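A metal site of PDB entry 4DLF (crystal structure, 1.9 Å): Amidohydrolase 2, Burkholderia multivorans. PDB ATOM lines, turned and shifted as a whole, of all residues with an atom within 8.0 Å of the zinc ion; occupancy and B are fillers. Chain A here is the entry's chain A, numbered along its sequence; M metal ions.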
ATOM      1  N   HIS A   9     -13.771  11.794 -16.914  1.00  0.00           N
ATOM      2  CA  HIS A   9     -13.390  12.654 -18.053  1.00  0.00           C
ATOM      3  C   HIS A   9     -12.834  13.993 -17.602  1.00  0.00           C
ATOM      4  O   HIS A   9     -13.606  14.840 -17.188  1.00  0.00           O
ATOM      5  CB  HIS A   9     -14.587  12.867 -18.997  1.00  0.00           C
ATOM      6  CG  HIS A   9     -14.274  13.645 -20.239  1.00  0.00           C
ATOM      7  ND1 HIS A   9     -14.144  13.060 -21.489  1.00  0.00           N
ATOM      8  CD2 HIS A   9     -14.078  14.977 -20.444  1.00  0.00           C
ATOM      9  CE1 HIS A   9     -13.879  13.996 -22.395  1.00  0.00           C
ATOM     10  NE2 HIS A   9     -13.830  15.173 -21.789  1.00  0.00           N
ATOM     11  N   GLN A  10     -11.520  14.197 -17.695  1.00  0.00           N
ATOM     12  CA  GLN A  10     -10.925  15.516 -17.445  1.00  0.00           C
ATOM     13  C   GLN A  10      -9.708  15.755 -18.336  1.00  0.00           C
ATOM     14  O   GLN A  10      -9.238  14.844 -19.025  1.00  0.00           O
ATOM     15  CB  GLN A  10     -10.562  15.740 -15.961  1.00  0.00           C
ATOM     16  CG  GLN A  10      -9.859  14.557 -15.265  1.00  0.00           C
ATOM     17  CD  GLN A  10      -8.343  14.514 -15.482  1.00  0.00           C
ATOM     18  OE1 GLN A  10      -7.701  13.491 -15.217  1.00  0.00           O
ATOM     19  NE2 GLN A  10      -7.774  15.620 -15.950  1.00  0.00           N
ATOM     20  N   HIS A  11      -9.210  16.991 -18.352  1.00  0.00           N
ATOM     21  CA  HIS A  11      -8.058  17.289 -19.190  1.00  0.00           C
ATOM     22  C   HIS A  11      -6.896  17.841 -18.381  1.00  0.00           C
ATOM     23  O   HIS A  11      -7.085  18.312 -17.256  1.00  0.00           O
ATOM     24  CB  HIS A  11      -8.461  18.240 -20.325  1.00  0.00           C
ATOM     25  CG  HIS A  11      -9.595  17.734 -21.148  1.00  0.00           C
ATOM     26  ND1 HIS A  11      -9.487  16.659 -21.996  1.00  0.00           N
ATOM     27  CD2 HIS A  11     -10.888  18.153 -21.241  1.00  0.00           C
ATOM     28  CE1 HIS A  11     -10.655  16.434 -22.581  1.00  0.00           C
ATOM     29  NE2 HIS A  11     -11.516  17.331 -22.137  1.00  0.00           N
ATOM     30  N   TRP A  13      -3.165  20.260 -19.244  1.00  0.00           N
ATOM     31  CA  TRP A  13      -2.339  20.917 -20.256  1.00  0.00           C
ATOM     32  C   TRP A  13      -1.364  21.949 -19.701  1.00  0.00           C
ATOM     33  O   TRP A  13      -1.629  22.587 -18.675  1.00  0.00           O
ATOM     34  CB  TRP A  13      -3.205  21.547 -21.370  1.00  0.00           C
ATOM     35  CG  TRP A  13      -4.194  22.621 -20.966  1.00  0.00           C
ATOM     36  CD1 TRP A  13      -3.904  23.897 -20.547  1.00  0.00           C
ATOM     37  CD2 TRP A  13      -5.620  22.541 -21.048  1.00  0.00           C
ATOM     38  NE1 TRP A  13      -5.064  24.593 -20.323  1.00  0.00           N
ATOM     39  CE2 TRP A  13      -6.135  23.788 -20.629  1.00  0.00           C
ATOM     40  CE3 TRP A  13      -6.517  21.533 -21.405  1.00  0.00           C
ATOM     41  CZ2 TRP A  13      -7.496  24.052 -20.561  1.00  0.00           C
ATOM     42  CZ3 TRP A  13      -7.878  21.797 -21.347  1.00  0.00           C
ATOM     43  CH2 TRP A  13      -8.351  23.042 -20.936  1.00  0.00           C
ATOM     44  N   TRP A  22      -9.120  25.208 -30.074  1.00  0.00           N
ATOM     45  CA  TRP A  22     -10.497  25.244 -29.587  1.00  0.00           C
ATOM     46  C   TRP A  22     -10.660  26.213 -28.420  1.00  0.00           C
ATOM     47  O   TRP A  22     -11.783  26.571 -28.067  1.00  0.00           O
ATOM     48  CB  TRP A  22     -11.023  23.828 -29.239  1.00  0.00           C
ATOM     49  CG  TRP A  22     -10.183  23.116 -28.255  1.00  0.00           C
ATOM     50  CD1 TRP A  22      -9.101  22.314 -28.525  1.00  0.00           C
ATOM     51  CD2 TRP A  22     -10.332  23.144 -26.841  1.00  0.00           C
ATOM     52  NE1 TRP A  22      -8.572  21.846 -27.344  1.00  0.00           N
ATOM     53  CE2 TRP A  22      -9.303  22.336 -26.300  1.00  0.00           C
ATOM     54  CE3 TRP A  22     -11.227  23.764 -25.965  1.00  0.00           C
ATOM     55  CZ2 TRP A  22      -9.154  22.126 -24.923  1.00  0.00           C
ATOM     56  CZ3 TRP A  22     -11.073  23.564 -24.596  1.00  0.00           C
ATOM     57  CH2 TRP A  22     -10.042  22.760 -24.094  1.00  0.00           C
ATOM     58  N   VAL A  54      -8.049  12.696 -20.534  1.00  0.00           N
ATOM     59  CA  VAL A  54      -8.420  12.517 -21.934  1.00  0.00           C
ATOM     60  C   VAL A  54      -7.653  13.497 -22.806  1.00  0.00           C
ATOM     61  O   VAL A  54      -7.523  14.675 -22.436  1.00  0.00           O
ATOM     62  CB  VAL A  54      -9.932  12.757 -22.119  1.00  0.00           C
ATOM     63  CG1 VAL A  54     -10.378  12.418 -23.559  1.00  0.00           C
ATOM     64  CG2 VAL A  54     -10.713  11.926 -21.112  1.00  0.00           C
ATOM     65  N   GLN A  55      -7.146  13.023 -23.942  1.00  0.00           N
ATOM     66  CA  GLN A  55      -6.413  13.874 -24.879  1.00  0.00           C
ATOM     67  C   GLN A  55      -7.157  15.178 -25.142  1.00  0.00           C
ATOM     68  O   GLN A  55      -8.385  15.172 -25.346  1.00  0.00           O
ATOM     69  CB  GLN A  55      -6.202  13.120 -26.203  1.00  0.00           C
ATOM     70  CG  GLN A  55      -7.523  12.695 -26.887  1.00  0.00           C
ATOM     71  CD  GLN A  55      -8.044  13.744 -27.878  1.00  0.00           C
ATOM     72  OE1 GLN A  55      -9.240  13.791 -28.175  1.00  0.00           O
ATOM     73  NE2 GLN A  55      -7.144  14.550 -28.408  1.00  0.00           N
ATOM     74  N   ALA A  56      -6.444  16.309 -25.086  1.00  0.00           N
ATOM     75  CA  ALA A  56      -7.098  17.603 -25.264  1.00  0.00           C
ATOM     76  C   ALA A  56      -6.658  18.228 -26.574  1.00  0.00           C
ATOM     77  O   ALA A  56      -7.115  19.318 -26.942  1.00  0.00           O
ATOM     78  CB  ALA A  56      -6.790  18.526 -24.104  1.00  0.00           C
ATOM     79  N   ARG A 106      -9.231   8.637 -28.419  1.00  0.00           N
ATOM     80  CA  ARG A 106     -10.299   9.522 -28.864  1.00  0.00           C
ATOM     81  C   ARG A 106      -9.819  10.361 -30.029  1.00  0.00           C
ATOM     82  O   ARG A 106      -8.680  10.828 -30.026  1.00  0.00           O
ATOM     83  CB  ARG A 106     -10.794  10.419 -27.725  1.00  0.00           C
ATOM     84  CG  ARG A 106     -11.957  11.340 -28.111  1.00  0.00           C
ATOM     85  CD  ARG A 106     -12.435  12.170 -26.917  1.00  0.00           C
ATOM     86  NE  ARG A 106     -11.675  13.406 -26.807  1.00  0.00           N
ATOM     87  CZ  ARG A 106     -12.077  14.477 -26.137  1.00  0.00           C
ATOM     88  NH1 ARG A 106     -11.316  15.561 -26.102  1.00  0.00           N
ATOM     89  NH2 ARG A 106     -13.250  14.468 -25.512  1.00  0.00           N
ATOM     90  N   LEU A 141     -16.656  11.619 -29.728  1.00  0.00           N
ATOM     91  CA  LEU A 141     -16.884  13.041 -29.465  1.00  0.00           C
ATOM     92  C   LEU A 141     -17.508  13.718 -30.692  1.00  0.00           C
ATOM     93  O   LEU A 141     -16.816  13.933 -31.717  1.00  0.00           O
ATOM     94  CB  LEU A 141     -15.572  13.752 -29.074  1.00  0.00           C
ATOM     95  CG  LEU A 141     -15.671  15.260 -28.926  1.00  0.00           C
ATOM     96  CD1 LEU A 141     -16.547  15.622 -27.732  1.00  0.00           C
ATOM     97  CD2 LEU A 141     -14.294  15.929 -28.817  1.00  0.00           C
ATOM     98  N   ASP A 165     -19.149  10.619 -25.526  1.00  0.00           N
ATOM     99  CA  ASP A 165     -18.738  11.783 -24.718  1.00  0.00           C
ATOM    100  C   ASP A 165     -19.815  12.832 -24.554  1.00  0.00           C
ATOM    101  O   ASP A 165     -20.527  13.155 -25.519  1.00  0.00           O
ATOM    102  CB  ASP A 165     -17.552  12.462 -25.365  1.00  0.00           C
ATOM    103  CG  ASP A 165     -16.261  11.881 -24.895  1.00  0.00           C
ATOM    104  OD1 ASP A 165     -16.317  10.863 -24.177  1.00  0.00           O
ATOM    105  OD2 ASP A 165     -15.211  12.433 -25.251  1.00  0.00           O
ATOM    106  N   HIS A 166     -19.932  13.362 -23.329  1.00  0.00           N
ATOM    107  CA  HIS A 166     -20.805  14.518 -23.060  1.00  0.00           C
ATOM    108  C   HIS A 166     -22.273  14.296 -23.431  1.00  0.00           C
ATOM    109  O   HIS A 166     -22.950  15.207 -23.891  1.00  0.00           O
ATOM    110  CB  HIS A 166     -20.251  15.746 -23.788  1.00  0.00           C
ATOM    111  CG  HIS A 166     -18.790  15.966 -23.559  1.00  0.00           C
ATOM    112  ND1 HIS A 166     -18.192  15.788 -22.324  1.00  0.00           N
ATOM    113  CD2 HIS A 166     -17.798  16.352 -24.398  1.00  0.00           C
ATOM    114  CE1 HIS A 166     -16.895  16.062 -22.421  1.00  0.00           C
ATOM    115  NE2 HIS A 166     -16.631  16.401 -23.670  1.00  0.00           N
ATOM    116  N   LYS A 169     -23.718  15.870 -26.507  1.00  0.00           N
ATOM    117  CA  LYS A 169     -23.830  17.326 -26.586  1.00  0.00           C
ATOM    118  C   LYS A 169     -25.176  17.867 -27.093  1.00  0.00           C
ATOM    119  O   LYS A 169     -25.250  18.431 -28.178  1.00  0.00           O
ATOM    120  CB  LYS A 169     -22.689  17.895 -27.428  1.00  0.00           C
ATOM    121  CG  LYS A 169     -21.349  17.805 -26.684  1.00  0.00           C
ATOM    122  CD  LYS A 169     -20.148  17.812 -27.629  1.00  0.00           C
ATOM    123  CE  LYS A 169     -19.608  19.216 -27.837  1.00  0.00           C
ATOM    124  NZ  LYS A 169     -18.190  19.390 -27.364  1.00  0.00           N
ATOM    125  N   LYS A 201     -21.207   9.083 -21.232  1.00  0.00           N
ATOM    126  CA  LYS A 201     -20.660   9.983 -20.222  1.00  0.00           C
ATOM    127  C   LYS A 201     -21.615  11.145 -19.938  1.00  0.00           C
ATOM    128  O   LYS A 201     -22.121  11.817 -20.856  1.00  0.00           O
ATOM    129  CB  LYS A 201     -19.278  10.511 -20.631  1.00  0.00           C
ATOM    130  CG  LYS A 201     -18.118   9.612 -20.242  1.00  0.00           C
ATOM    131  CD  LYS A 201     -16.826  10.107 -20.911  1.00  0.00           C
ATOM    132  CE  LYS A 201     -15.611   9.280 -20.481  1.00  0.00           C
ATOM    133  NZ  LYS A 201     -14.374   9.768 -21.194  1.00  0.00           N
ATOM    134  N   SER A 203     -21.276  14.459 -18.633  1.00  0.00           N
ATOM    135  CA  SER A 203     -20.204  15.413 -18.413  1.00  0.00           C
ATOM    136  C   SER A 203     -20.326  16.444 -19.523  1.00  0.00           C
ATOM    137  O   SER A 203     -21.024  16.201 -20.515  1.00  0.00           O
ATOM    138  CB  SER A 203     -18.869  14.708 -18.547  1.00  0.00           C
ATOM    139  OG  SER A 203     -18.817  14.021 -19.782  1.00  0.00           O
ATOM    140  N   GLY A 204     -19.681  17.597 -19.367  1.00  0.00           N
ATOM    141  CA  GLY A 204     -19.673  18.577 -20.435  1.00  0.00           C
ATOM    142  C   GLY A 204     -21.028  19.165 -20.766  1.00  0.00           C
ATOM    143  O   GLY A 204     -21.247  19.614 -21.901  1.00  0.00           O
ATOM    144  N   THR A 207     -21.336  23.417 -20.320  1.00  0.00           N
ATOM    145  CA  THR A 207     -20.739  24.204 -21.393  1.00  0.00           C
ATOM    146  C   THR A 207     -21.477  24.156 -22.730  1.00  0.00           C
ATOM    147  O   THR A 207     -21.129  24.906 -23.660  1.00  0.00           O
ATOM    148  CB  THR A 207     -19.262  23.866 -21.613  1.00  0.00           C
ATOM    149  OG1 THR A 207     -19.063  22.441 -21.595  1.00  0.00           O
ATOM    150  CG2 THR A 207     -18.416  24.504 -20.521  1.00  0.00           C
ATOM    151  N   SER A 243     -16.205  15.248 -15.043  1.00  0.00           N
ATOM    152  CA  SER A 243     -16.336  16.675 -14.744  1.00  0.00           C
ATOM    153  C   SER A 243     -16.161  17.545 -15.994  1.00  0.00           C
ATOM    154  O   SER A 243     -16.726  18.648 -16.076  1.00  0.00           O
ATOM    155  CB  SER A 243     -15.294  17.082 -13.715  1.00  0.00           C
ATOM    156  OG  SER A 243     -13.980  16.955 -14.245  1.00  0.00           O
ATOM    157  N   ASP A 244     -15.381  17.048 -16.936  1.00  0.00           N
ATOM    158  CA  ASP A 244     -14.841  17.818 -18.054  1.00  0.00           C
ATOM    159  C   ASP A 244     -14.024  19.030 -17.570  1.00  0.00           C
ATOM    160  O   ASP A 244     -13.864  20.012 -18.296  1.00  0.00           O
ATOM    161  CB  ASP A 244     -15.920  18.242 -19.061  1.00  0.00           C
ATOM    162  CG  ASP A 244     -15.346  18.643 -20.396  1.00  0.00           C
ATOM    163  OD1 ASP A 244     -14.366  17.994 -20.847  1.00  0.00           O
ATOM    164  OD2 ASP A 244     -15.850  19.646 -20.967  1.00  0.00           O
ATOM    165  N   TRP A 245     -13.489  18.941 -16.360  1.00  0.00           N
ATOM    166  CA  TRP A 245     -12.513  19.941 -15.898  1.00  0.00           C
ATOM    167  C   TRP A 245     -11.255  19.843 -16.761  1.00  0.00           C
ATOM    168  O   TRP A 245     -10.858  18.743 -17.182  1.00  0.00           O
ATOM    169  CB  TRP A 245     -12.173  19.643 -14.438  1.00  0.00           C
ATOM    170  CG  TRP A 245     -11.199  20.588 -13.781  1.00  0.00           C
ATOM    171  CD1 TRP A 245     -11.494  21.699 -13.051  1.00  0.00           C
ATOM    172  CD2 TRP A 245      -9.775  20.451 -13.752  1.00  0.00           C
ATOM    173  NE1 TRP A 245     -10.329  22.269 -12.572  1.00  0.00           N
ATOM    174  CE2 TRP A 245      -9.267  21.523 -12.988  1.00  0.00           C
ATOM    175  CE3 TRP A 245      -8.870  19.520 -14.297  1.00  0.00           C
ATOM    176  CZ2 TRP A 245      -7.886  21.697 -12.759  1.00  0.00           C
ATOM    177  CZ3 TRP A 245      -7.508  19.700 -14.068  1.00  0.00           C
ATOM    178  CH2 TRP A 245      -7.032  20.773 -13.306  1.00  0.00           C
ATOM    179  N   PRO A 246     -10.611  20.995 -17.038  1.00  0.00           N
ATOM    180  CA  PRO A 246     -10.933  22.368 -16.625  1.00  0.00           C
ATOM    181  C   PRO A 246     -11.907  23.097 -17.544  1.00  0.00           C
ATOM    182  O   PRO A 246     -12.312  24.231 -17.210  1.00  0.00           O
ATOM    183  CB  PRO A 246      -9.566  23.060 -16.675  1.00  0.00           C
ATOM    184  CG  PRO A 246      -8.799  22.310 -17.694  1.00  0.00           C
ATOM    185  CD  PRO A 246      -9.296  20.894 -17.686  1.00  0.00           C
ATOM    186  N   VAL A 247     -12.279  22.479 -18.666  1.00  0.00           N
ATOM    187  CA  VAL A 247     -13.202  23.109 -19.613  1.00  0.00           C
ATOM    188  C   VAL A 247     -14.509  23.594 -18.985  1.00  0.00           C
ATOM    189  O   VAL A 247     -15.042  24.648 -19.372  1.00  0.00           O
ATOM    190  CB  VAL A 247     -13.476  22.191 -20.830  1.00  0.00           C
ATOM    191  CG1 VAL A 247     -14.442  22.849 -21.796  1.00  0.00           C
ATOM    192  CG2 VAL A 247     -12.156  21.885 -21.559  1.00  0.00           C
ATOM    193  N   CYS A 248     -14.998  22.872 -17.970  1.00  0.00           N
ATOM    194  CA  CYS A 248     -16.275  23.230 -17.344  1.00  0.00           C
ATOM    195  C   CYS A 248     -16.199  24.579 -16.648  1.00  0.00           C
ATOM    196  O   CYS A 248     -17.235  25.207 -16.393  1.00  0.00           O
ATOM    197  CB  CYS A 248     -16.679  22.178 -16.307  1.00  0.00           C
ATOM    198  SG  CYS A 248     -15.475  22.042 -14.971  1.00  0.00           S
HETATM  199 ZN    ZN M   1     -13.557  17.232 -22.489  1.00  0.00          ZN
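O of Val 54 is in hydrogen-bond range of ND1 of His 11, at 2.8 Å.
The backbone NH (N) of His 11 is in hydrogen-bond range of the backbone carbonyl oxygen (O) of Trp 245 (2.7 Å).
The backbone NH (N) of Ser 243 lies within hydrogen-bond range of the backbone carbonyl oxygen (O) of His 9 (3.4 Å).
A ring nitrogen (ND1) of His 9 sits at hydrogen-bond distance from the side-chain amino group of Lys 201, at 3.3 Å.
OG of Ser 203 sits at hydrogen-bond distance from ND1 of His 166 (3.2 Å).
The zinc ion is bound by OD1 of Asp 244, at 2.0 Å.
NE2 of His 11 is bound to the zinc ion, 2.1 Å away.
The zinc ion is bound by a ring nitrogen (NE2) of His 9 (2.2 Å).
The zinc ion has three donor atoms within binding distance.
NE2 of His 166 touches the zinc ion (3.4 Å).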
